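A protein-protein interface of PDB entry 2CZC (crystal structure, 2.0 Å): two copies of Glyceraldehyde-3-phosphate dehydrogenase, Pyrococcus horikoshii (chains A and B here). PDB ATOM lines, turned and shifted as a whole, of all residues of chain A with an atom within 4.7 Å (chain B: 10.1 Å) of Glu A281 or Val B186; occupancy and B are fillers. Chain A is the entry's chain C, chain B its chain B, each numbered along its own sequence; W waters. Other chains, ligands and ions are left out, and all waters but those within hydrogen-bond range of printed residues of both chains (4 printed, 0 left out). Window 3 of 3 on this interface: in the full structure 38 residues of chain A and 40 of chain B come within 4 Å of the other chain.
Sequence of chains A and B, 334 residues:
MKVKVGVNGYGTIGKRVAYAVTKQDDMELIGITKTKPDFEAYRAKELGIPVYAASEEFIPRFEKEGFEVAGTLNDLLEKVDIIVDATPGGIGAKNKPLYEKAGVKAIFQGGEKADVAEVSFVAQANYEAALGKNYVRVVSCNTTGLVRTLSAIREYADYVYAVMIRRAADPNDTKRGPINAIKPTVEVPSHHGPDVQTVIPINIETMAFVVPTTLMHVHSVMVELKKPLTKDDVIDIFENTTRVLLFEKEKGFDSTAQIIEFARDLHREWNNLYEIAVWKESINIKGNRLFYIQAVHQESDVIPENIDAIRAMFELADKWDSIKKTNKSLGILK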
ATOM      1  N   PHE A 247      26.661 -11.056  -6.793  1.00  0.00           N
ATOM      2  CA  PHE A 247      26.643 -12.097  -7.822  1.00  0.00           C
ATOM      3  C   PHE A 247      25.820 -13.288  -7.336  1.00  0.00           C
ATOM      4  O   PHE A 247      25.888 -13.673  -6.161  1.00  0.00           O
ATOM      5  CB  PHE A 247      28.058 -12.582  -8.146  1.00  0.00           C
ATOM      6  CG  PHE A 247      28.886 -11.581  -8.920  1.00  0.00           C
ATOM      7  CD1 PHE A 247      29.495 -10.511  -8.279  1.00  0.00           C
ATOM      8  CD2 PHE A 247      29.057 -11.721 -10.290  1.00  0.00           C
ATOM      9  CE1 PHE A 247      30.269  -9.588  -8.990  1.00  0.00           C
ATOM     10  CE2 PHE A 247      29.836 -10.801 -11.018  1.00  0.00           C
ATOM     11  CZ  PHE A 247      30.440  -9.736 -10.368  1.00  0.00           C
ATOM     12  N   GLU A 248      25.035 -13.871  -8.231  1.00  0.00           N
ATOM     13  CA  GLU A 248      24.235 -15.028  -7.864  1.00  0.00           C
ATOM     14  C   GLU A 248      24.854 -16.338  -8.342  1.00  0.00           C
ATOM     15  O   GLU A 248      25.136 -16.530  -9.530  1.00  0.00           O
ATOM     16  CB  GLU A 248      22.816 -14.913  -8.434  1.00  0.00           C
ATOM     17  CG  GLU A 248      22.072 -13.681  -7.984  1.00  0.00           C
ATOM     18  CD  GLU A 248      20.680 -13.612  -8.587  1.00  0.00           C
ATOM     19  OE1 GLU A 248      20.242 -12.490  -8.931  1.00  0.00           O
ATOM     20  OE2 GLU A 248      20.028 -14.680  -8.707  1.00  0.00           O
ATOM     21  N   LYS A 249      25.064 -17.243  -7.400  1.00  0.00           N
ATOM     22  CA  LYS A 249      25.596 -18.565  -7.698  1.00  0.00           C
ATOM     23  C   LYS A 249      24.573 -19.225  -8.645  1.00  0.00           C
ATOM     24  O   LYS A 249      24.938 -19.942  -9.558  1.00  0.00           O
ATOM     25  CB  LYS A 249      25.707 -19.350  -6.384  1.00  0.00           C
ATOM     26  CG  LYS A 249      26.563 -20.603  -6.402  1.00  0.00           C
ATOM     27  CD  LYS A 249      25.927 -21.714  -7.188  1.00  0.00           C
ATOM     28  CE  LYS A 249      26.693 -23.033  -7.002  1.00  0.00           C
ATOM     29  NZ  LYS A 249      26.730 -23.491  -5.582  1.00  0.00           N
ATOM     30  N   GLU A 250      23.290 -18.960  -8.427  1.00  0.00           N
ATOM     31  CA  GLU A 250      22.234 -19.550  -9.260  1.00  0.00           C
ATOM     32  C   GLU A 250      22.287 -19.108 -10.728  1.00  0.00           C
ATOM     33  O   GLU A 250      21.690 -19.748 -11.601  1.00  0.00           O
ATOM     34  CB  GLU A 250      20.848 -19.240  -8.673  1.00  0.00           C
ATOM     35  CG  GLU A 250      20.593 -19.911  -7.328  1.00  0.00           C
ATOM     36  CD  GLU A 250      20.968 -21.387  -7.342  1.00  0.00           C
ATOM     37  OE1 GLU A 250      20.559 -22.101  -8.283  1.00  0.00           O
ATOM     38  OE2 GLU A 250      21.673 -21.837  -6.411  1.00  0.00           O
ATOM     39  N   TRP A 279      28.644 -12.881  -2.893  1.00  0.00           N
ATOM     40  CA  TRP A 279      27.696 -13.894  -3.342  1.00  0.00           C
ATOM     41  C   TRP A 279      26.357 -13.632  -2.637  1.00  0.00           C
ATOM     42  O   TRP A 279      26.212 -13.808  -1.426  1.00  0.00           O
ATOM     43  CB  TRP A 279      28.233 -15.288  -3.029  1.00  0.00           C
ATOM     44  CG  TRP A 279      29.114 -15.841  -4.100  1.00  0.00           C
ATOM     45  CD1 TRP A 279      28.703 -16.456  -5.250  1.00  0.00           C
ATOM     46  CD2 TRP A 279      30.552 -15.853  -4.128  1.00  0.00           C
ATOM     47  NE1 TRP A 279      29.790 -16.855  -5.985  1.00  0.00           N
ATOM     48  CE2 TRP A 279      30.937 -16.498  -5.326  1.00  0.00           C
ATOM     49  CE3 TRP A 279      31.552 -15.382  -3.257  1.00  0.00           C
ATOM     50  CZ2 TRP A 279      32.283 -16.692  -5.683  1.00  0.00           C
ATOM     51  CZ3 TRP A 279      32.901 -15.575  -3.617  1.00  0.00           C
ATOM     52  CH2 TRP A 279      33.245 -16.227  -4.819  1.00  0.00           C
ATOM     53  N   LYS A 280      25.376 -13.188  -3.409  1.00  0.00           N
ATOM     54  CA  LYS A 280      24.062 -12.880  -2.864  1.00  0.00           C
ATOM     55  C   LYS A 280      23.506 -14.025  -2.025  1.00  0.00           C
ATOM     56  O   LYS A 280      23.005 -13.822  -0.909  1.00  0.00           O
ATOM     57  CB  LYS A 280      23.086 -12.569  -3.997  1.00  0.00           C
ATOM     58  CG  LYS A 280      21.700 -12.149  -3.517  1.00  0.00           C
ATOM     59  CD  LYS A 280      20.854 -11.674  -4.679  1.00  0.00           C
ATOM     60  CE  LYS A 280      19.536 -11.093  -4.188  1.00  0.00           C
ATOM     61  NZ  LYS A 280      18.726 -10.581  -5.320  1.00  0.00           N
ATOM     62  N   GLU A 281      23.582 -15.232  -2.566  1.00  0.00           N
ATOM     63  CA  GLU A 281      23.061 -16.389  -1.855  1.00  0.00           C
ATOM     64  C   GLU A 281      23.798 -16.664  -0.543  1.00  0.00           C
ATOM     65  O   GLU A 281      23.273 -17.385   0.329  1.00  0.00           O
ATOM     66  CB  GLU A 281      23.123 -17.649  -2.728  1.00  0.00           C
ATOM     67  CG  GLU A 281      22.329 -17.602  -4.023  1.00  0.00           C
ATOM     68  CD  GLU A 281      23.139 -17.068  -5.174  1.00  0.00           C
ATOM     69  OE1 GLU A 281      22.797 -17.426  -6.316  1.00  0.00           O
ATOM     70  OE2 GLU A 281      24.100 -16.301  -4.925  1.00  0.00           O
ATOM     71  N   SER A 282      24.989 -16.093  -0.368  1.00  0.00           N
ATOM     72  CA  SER A 282      25.738 -16.365   0.848  1.00  0.00           C
ATOM     73  C   SER A 282      25.286 -15.547   2.050  1.00  0.00           C
ATOM     74  O   SER A 282      25.574 -15.910   3.181  1.00  0.00           O
ATOM     75  CB  SER A 282      27.240 -16.156   0.629  1.00  0.00           C
ATOM     76  OG  SER A 282      27.588 -14.784   0.628  1.00  0.00           O
ATOM     77  N   ILE A 283      24.581 -14.451   1.804  1.00  0.00           N
ATOM     78  CA  ILE A 283      24.118 -13.598   2.891  1.00  0.00           C
ATOM     79  C   ILE A 283      23.045 -14.294   3.728  1.00  0.00           C
ATOM     80  O   ILE A 283      21.997 -14.687   3.221  1.00  0.00           O
ATOM     81  CB  ILE A 283      23.558 -12.277   2.329  1.00  0.00           C
ATOM     82  CG1 ILE A 283      24.640 -11.602   1.472  1.00  0.00           C
ATOM     83  CG2 ILE A 283      23.134 -11.345   3.480  1.00  0.00           C
ATOM     84  CD1 ILE A 283      24.130 -10.444   0.627  1.00  0.00           C
ATOM     85  N   ILE A 293      29.859 -14.100   2.133  1.00  0.00           N
ATOM     86  CA  ILE A 293      31.125 -14.421   1.487  1.00  0.00           C
ATOM     87  C   ILE A 293      31.351 -13.418   0.364  1.00  0.00           C
ATOM     88  O   ILE A 293      30.437 -13.128  -0.401  1.00  0.00           O
ATOM     89  CB  ILE A 293      31.076 -15.837   0.891  1.00  0.00           C
ATOM     90  CG1 ILE A 293      30.658 -16.849   1.976  1.00  0.00           C
ATOM     91  CG2 ILE A 293      32.424 -16.215   0.308  1.00  0.00           C
ATOM     92  CD1 ILE A 293      30.536 -18.281   1.476  1.00  0.00           C
ATOM     93  N   ILE B 182      38.645 -20.424  -6.303  1.00  0.00           N
ATOM     94  CA  ILE B 182      38.178 -20.695  -4.946  1.00  0.00           C
ATOM     95  C   ILE B 182      36.655 -20.828  -5.116  1.00  0.00           C
ATOM     96  O   ILE B 182      35.999 -19.934  -5.632  1.00  0.00           O
ATOM     97  CB  ILE B 182      38.506 -19.560  -3.966  1.00  0.00           C
ATOM     98  CG1 ILE B 182      40.032 -19.490  -3.748  1.00  0.00           C
ATOM     99  CG2 ILE B 182      37.765 -19.822  -2.614  1.00  0.00           C
ATOM    100  CD1 ILE B 182      40.480 -18.287  -2.970  1.00  0.00           C
ATOM    101  N   LYS B 183      36.119 -21.974  -4.719  1.00  0.00           N
ATOM    102  CA  LYS B 183      34.699 -22.262  -4.854  1.00  0.00           C
ATOM    103  C   LYS B 183      34.055 -22.232  -3.492  1.00  0.00           C
ATOM    104  O   LYS B 183      34.268 -23.118  -2.671  1.00  0.00           O
ATOM    105  CB  LYS B 183      34.516 -23.643  -5.492  1.00  0.00           C
ATOM    106  CG  LYS B 183      33.080 -24.040  -5.783  1.00  0.00           C
ATOM    107  CD  LYS B 183      33.032 -25.496  -6.273  1.00  0.00           C
ATOM    108  CE  LYS B 183      31.648 -25.896  -6.718  1.00  0.00           C
ATOM    109  NZ  LYS B 183      30.656 -25.680  -5.640  1.00  0.00           N
ATOM    110  N   PRO B 184      33.229 -21.212  -3.238  1.00  0.00           N
ATOM    111  CA  PRO B 184      32.583 -21.134  -1.930  1.00  0.00           C
ATOM    112  C   PRO B 184      31.304 -21.930  -1.854  1.00  0.00           C
ATOM    113  O   PRO B 184      30.607 -22.093  -2.862  1.00  0.00           O
ATOM    114  CB  PRO B 184      32.291 -19.658  -1.796  1.00  0.00           C
ATOM    115  CG  PRO B 184      31.850 -19.308  -3.241  1.00  0.00           C
ATOM    116  CD  PRO B 184      32.841 -20.072  -4.103  1.00  0.00           C
ATOM    117  N   THR B 185      30.998 -22.429  -0.661  1.00  0.00           N
ATOM    118  CA  THR B 185      29.742 -23.106  -0.444  1.00  0.00           C
ATOM    119  C   THR B 185      28.844 -21.939  -0.008  1.00  0.00           C
ATOM    120  O   THR B 185      29.087 -21.307   1.021  1.00  0.00           O
ATOM    121  CB  THR B 185      29.859 -24.158   0.678  1.00  0.00           C
ATOM    122  OG1 THR B 185      30.596 -25.283   0.184  1.00  0.00           O
ATOM    123  CG2 THR B 185      28.480 -24.614   1.141  1.00  0.00           C
ATOM    124  N   VAL B 186      27.834 -21.623  -0.810  1.00  0.00           N
ATOM    125  CA  VAL B 186      26.963 -20.505  -0.488  1.00  0.00           C
ATOM    126  C   VAL B 186      25.939 -20.826   0.578  1.00  0.00           C
ATOM    127  O   VAL B 186      25.342 -19.911   1.151  1.00  0.00           O
ATOM    128  CB  VAL B 186      26.260 -19.959  -1.743  1.00  0.00           C
ATOM    129  CG1 VAL B 186      27.302 -19.380  -2.676  1.00  0.00           C
ATOM    130  CG2 VAL B 186      25.479 -21.064  -2.451  1.00  0.00           C
ATOM    131  N   GLU B 187      25.736 -22.114   0.848  1.00  0.00           N
ATOM    132  CA  GLU B 187      24.804 -22.520   1.887  1.00  0.00           C
ATOM    133  C   GLU B 187      25.476 -22.166   3.209  1.00  0.00           C
ATOM    134  O   GLU B 187      26.490 -22.756   3.596  1.00  0.00           O
ATOM    135  CB  GLU B 187      24.511 -24.023   1.818  1.00  0.00           C
ATOM    136  CG  GLU B 187      23.644 -24.425   0.638  1.00  0.00           C
ATOM    137  CD  GLU B 187      24.351 -24.275  -0.707  1.00  0.00           C
ATOM    138  OE1 GLU B 187      23.661 -23.981  -1.712  1.00  0.00           O
ATOM    139  OE2 GLU B 187      25.586 -24.465  -0.767  1.00  0.00           O
ATOM    140  N   VAL B 188      24.913 -21.172   3.885  1.00  0.00           N
ATOM    141  CA  VAL B 188      25.450 -20.705   5.153  1.00  0.00           C
ATOM    142  C   VAL B 188      24.336 -20.596   6.172  1.00  0.00           C
ATOM    143  O   VAL B 188      23.319 -19.946   5.923  1.00  0.00           O
ATOM    144  CB  VAL B 188      26.081 -19.313   5.012  1.00  0.00           C
ATOM    145  CG1 VAL B 188      26.726 -18.911   6.327  1.00  0.00           C
ATOM    146  CG2 VAL B 188      27.085 -19.306   3.875  1.00  0.00           C
ATOM    147  N   PRO B 189      24.509 -21.231   7.339  1.00  0.00           N
ATOM    148  CA  PRO B 189      25.677 -22.027   7.729  1.00  0.00           C
ATOM    149  C   PRO B 189      25.868 -23.307   6.913  1.00  0.00           C
ATOM    150  O   PRO B 189      24.931 -23.813   6.294  1.00  0.00           O
ATOM    151  CB  PRO B 189      25.418 -22.307   9.209  1.00  0.00           C
ATOM    152  CG  PRO B 189      24.651 -21.075   9.646  1.00  0.00           C
ATOM    153  CD  PRO B 189      23.672 -20.918   8.509  1.00  0.00           C
ATOM    154  N   SER B 190      27.102 -23.806   6.913  1.00  0.00           N
ATOM    155  CA  SER B 190      27.503 -25.017   6.194  1.00  0.00           C
ATOM    156  C   SER B 190      26.928 -26.253   6.882  1.00  0.00           C
ATOM    157  O   SER B 190      26.444 -26.159   8.005  1.00  0.00           O
ATOM    158  CB  SER B 190      29.034 -25.107   6.167  1.00  0.00           C
ATOM    159  OG  SER B 190      29.482 -26.321   5.611  1.00  0.00           O
ATOM    160  N   HIS B 191      26.999 -27.410   6.231  1.00  0.00           N
ATOM    161  CA  HIS B 191      26.447 -28.629   6.819  1.00  0.00           C
ATOM    162  C   HIS B 191      27.403 -29.325   7.786  1.00  0.00           C
ATOM    163  O   HIS B 191      27.033 -30.287   8.459  1.00  0.00           O
ATOM    164  CB  HIS B 191      26.035 -29.605   5.720  1.00  0.00           C
ATOM    165  CG  HIS B 191      27.187 -30.137   4.938  1.00  0.00           C
ATOM    166  ND1 HIS B 191      28.009 -31.142   5.405  1.00  0.00           N
ATOM    167  CD2 HIS B 191      27.699 -29.757   3.745  1.00  0.00           C
ATOM    168  CE1 HIS B 191      28.981 -31.353   4.533  1.00  0.00           C
ATOM    169  NE2 HIS B 191      28.816 -30.524   3.517  1.00  0.00           N
ATOM    170  N   THR B 206      29.384 -23.395  10.710  1.00  0.00           N
ATOM    171  CA  THR B 206      30.527 -23.521   9.824  1.00  0.00           C
ATOM    172  C   THR B 206      30.249 -22.987   8.434  1.00  0.00           C
ATOM    173  O   THR B 206      29.102 -22.775   8.060  1.00  0.00           O
ATOM    174  CB  THR B 206      30.925 -25.001   9.689  1.00  0.00           C
ATOM    175  OG1 THR B 206      29.790 -25.747   9.219  1.00  0.00           O
ATOM    176  CG2 THR B 206      31.365 -25.557  11.040  1.00  0.00           C
ATOM    177  N   MET B 207      31.317 -22.767   7.681  1.00  0.00           N
ATOM    178  CA  MET B 207      31.229 -22.294   6.309  1.00  0.00           C
ATOM    179  C   MET B 207      32.369 -22.998   5.590  1.00  0.00           C
ATOM    180  O   MET B 207      33.444 -23.218   6.170  1.00  0.00           O
ATOM    181  CB  MET B 207      31.352 -20.770   6.248  1.00  0.00           C
ATOM    182  CG  MET B 207      30.015 -20.067   6.502  1.00  0.00           C
ATOM    183  SD  MET B 207      30.094 -18.252   6.665  1.00  0.00           S
ATOM    184  CE  MET B 207      31.102 -17.847   5.173  1.00  0.00           C
ATOM    185  N   ALA B 208      32.139 -23.385   4.338  1.00  0.00           N
ATOM    186  CA  ALA B 208      33.152 -24.130   3.612  1.00  0.00           C
ATOM    187  C   ALA B 208      33.508 -23.584   2.241  1.00  0.00           C
ATOM    188  O   ALA B 208      32.696 -22.934   1.572  1.00  0.00           O
ATOM    189  CB  ALA B 208      32.722 -25.581   3.497  1.00  0.00           C
ATOM    190  N   PHE B 209      34.729 -23.899   1.832  1.00  0.00           N
ATOM    191  CA  PHE B 209      35.296 -23.450   0.572  1.00  0.00           C
ATOM    192  C   PHE B 209      36.190 -24.551   0.004  1.00  0.00           C
ATOM    193  O   PHE B 209      36.719 -25.381   0.747  1.00  0.00           O
ATOM    194  CB  PHE B 209      36.157 -22.214   0.831  1.00  0.00           C
ATOM    195  CG  PHE B 209      35.412 -21.070   1.467  1.00  0.00           C
ATOM    196  CD1 PHE B 209      34.852 -20.067   0.685  1.00  0.00           C
ATOM    197  CD2 PHE B 209      35.235 -21.015   2.850  1.00  0.00           C
ATOM    198  CE1 PHE B 209      34.121 -19.031   1.262  1.00  0.00           C
ATOM    199  CE2 PHE B 209      34.504 -19.977   3.438  1.00  0.00           C
ATOM    200  CZ  PHE B 209      33.944 -18.984   2.637  1.00  0.00           C
ATOM    201  N   VAL B 210      36.357 -24.559  -1.307  1.00  0.00           N
ATOM    202  CA  VAL B 210      37.227 -25.527  -1.973  1.00  0.00           C
ATOM    203  C   VAL B 210      38.322 -24.727  -2.693  1.00  0.00           C
ATOM    204  O   VAL B 210      38.027 -23.722  -3.354  1.00  0.00           O
ATOM    205  CB  VAL B 210      36.439 -26.345  -3.007  1.00  0.00           C
ATOM    206  CG1 VAL B 210      37.383 -27.202  -3.827  1.00  0.00           C
ATOM    207  CG2 VAL B 210      35.411 -27.225  -2.295  1.00  0.00           C
HETATM  208  O   HOH W   1      29.828 -22.849  -5.356  1.00  0.00           O
HETATM  209  O   HOH W   2      24.129 -23.858  -4.335  1.00  0.00           O
HETATM  210  O   HOH W   3      27.810 -26.589  -6.155  1.00  0.00           O
HETATM  211  O   HOH W   4      27.229 -23.440  -2.776  1.00  0.00           O
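The backbone carbonyl oxygen (O) of Glu A281 lies close to the backbone carbonyl oxygen (O) of Val B186 (3.4 Å).
The backbone NH (N) of Thr B185 is in hydrogen-bond range of the backbone carbonyl oxygen (O) of Ala B208 (2.9 Å). OE1 of Glu A281 lies within hydrogen-bond range of N of Lys A249, 2.5 Å away. N of Glu A250 is in hydrogen-bond range of OE1 of Glu A281. The backbone carbonyl oxygen of Trp A279 lies within hydrogen-bond range of the side-chain hydroxyl of Ser A282, 2.7 Å away. The backbone carbonyl oxygen of Ile A293 lies within hydrogen-bond range of the backbone NH of Trp A279 (3.1 Å). The backbone NH of Ile A293 lies within hydrogen-bond range of the side-chain hydroxyl of Ser A282.
Among the printed residues, merely in contact across the chains: Ile A293 with Met B207, Ile A293 with Thr B185, Ile A293 with Phe B209, Ser A282 with Val B186, Trp A279 with Pro B184, Ser A282 with Val B188, Ile A293 with Pro B184 and Lys A249 with Val B186.
Printed residues of chain B within 4 Å of Lys A249: Val B186. No residue of chain B comes within 4 Å of Glu A250. Printed residues of chain B within 4 Å of Trp A279: Pro B184 (3.6 Å). Lys A280 touches none of the printed residues of chain B. Glu A281 touches just one residue of chain B: Val B186. Ser A282 touches just these residues of chain B: Val B186 and Val B188. Printed residues of chain B within 4 Å of Ile A293: Pro B184 (3.96 Å), Thr B185 (3.4 Å), Met B207 (3.4 Å) and Phe B209 (3.4 Å). Printed residues of chain A within 4 Å of Val B186: Lys A249 (3.99 Å), Glu A281 (3.4 Å) and Ser A282 (3.6 Å). Of the printed residues of chain A, Val B188 touches Ser A282. Ala B208 touches none of the printed residues of chain A. Of the printed residues of chain A, Phe B209 touches Ile A293. The nearest residue of chain B that does not touch Glu A281 is Glu B187 (5.4 Å). The nearest printed residue of chain A that does not touch Val B188 is Ile A293 (4.3 Å).
Printed residues of chain A that touch a printed residue of chain B: Lys A249, Trp A279, Glu A281, Ser A282 and Ile A293. Of the 15 printed residues of chain B, 6 touch a printed residue of chain A. Printed residues of chain B that touch a printed residue of chain A: Pro B184, Thr B185, Val B186, Val B188, Met B207 and Phe B209. Hydrophobic or aromatic side chains of chain B within 4 Å of the printed part of chain A: Pro B184, Val B186, Val B188, Met B207 and Phe B209. Among the printed residues, no Asp or Glu carboxylate lies within 4 Å of a Lys or Arg side-chain nitrogen of the other chain.
No position is printed for both chains. Of the 9 pairs that touch across the chains among the printed residues, none has its exchanged pair printed and touching as well.
Water W2 lies within hydrogen-bond range of the side-chain carboxylate (OE1) of Glu B187 and the side-chain amino group (NZ) of Lys A249. Water W1 lies within hydrogen-bond range of O of Pro B184 (2.7 Å), NZ of Lys B183 (3.0 Å) and NZ of Lys A249 (3.2 Å). Water W4 lies within hydrogen-bond range of the backbone NH (N) of Val B186, the side-chain carboxylate (OE2) of Glu B187 and the side-chain amino group (NZ) of Lys A249. Water W3 lies within hydrogen-bond range of the side-chain amino group (NZ) of Lys B183 and the side-chain amino group (NZ) of Lys A249.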
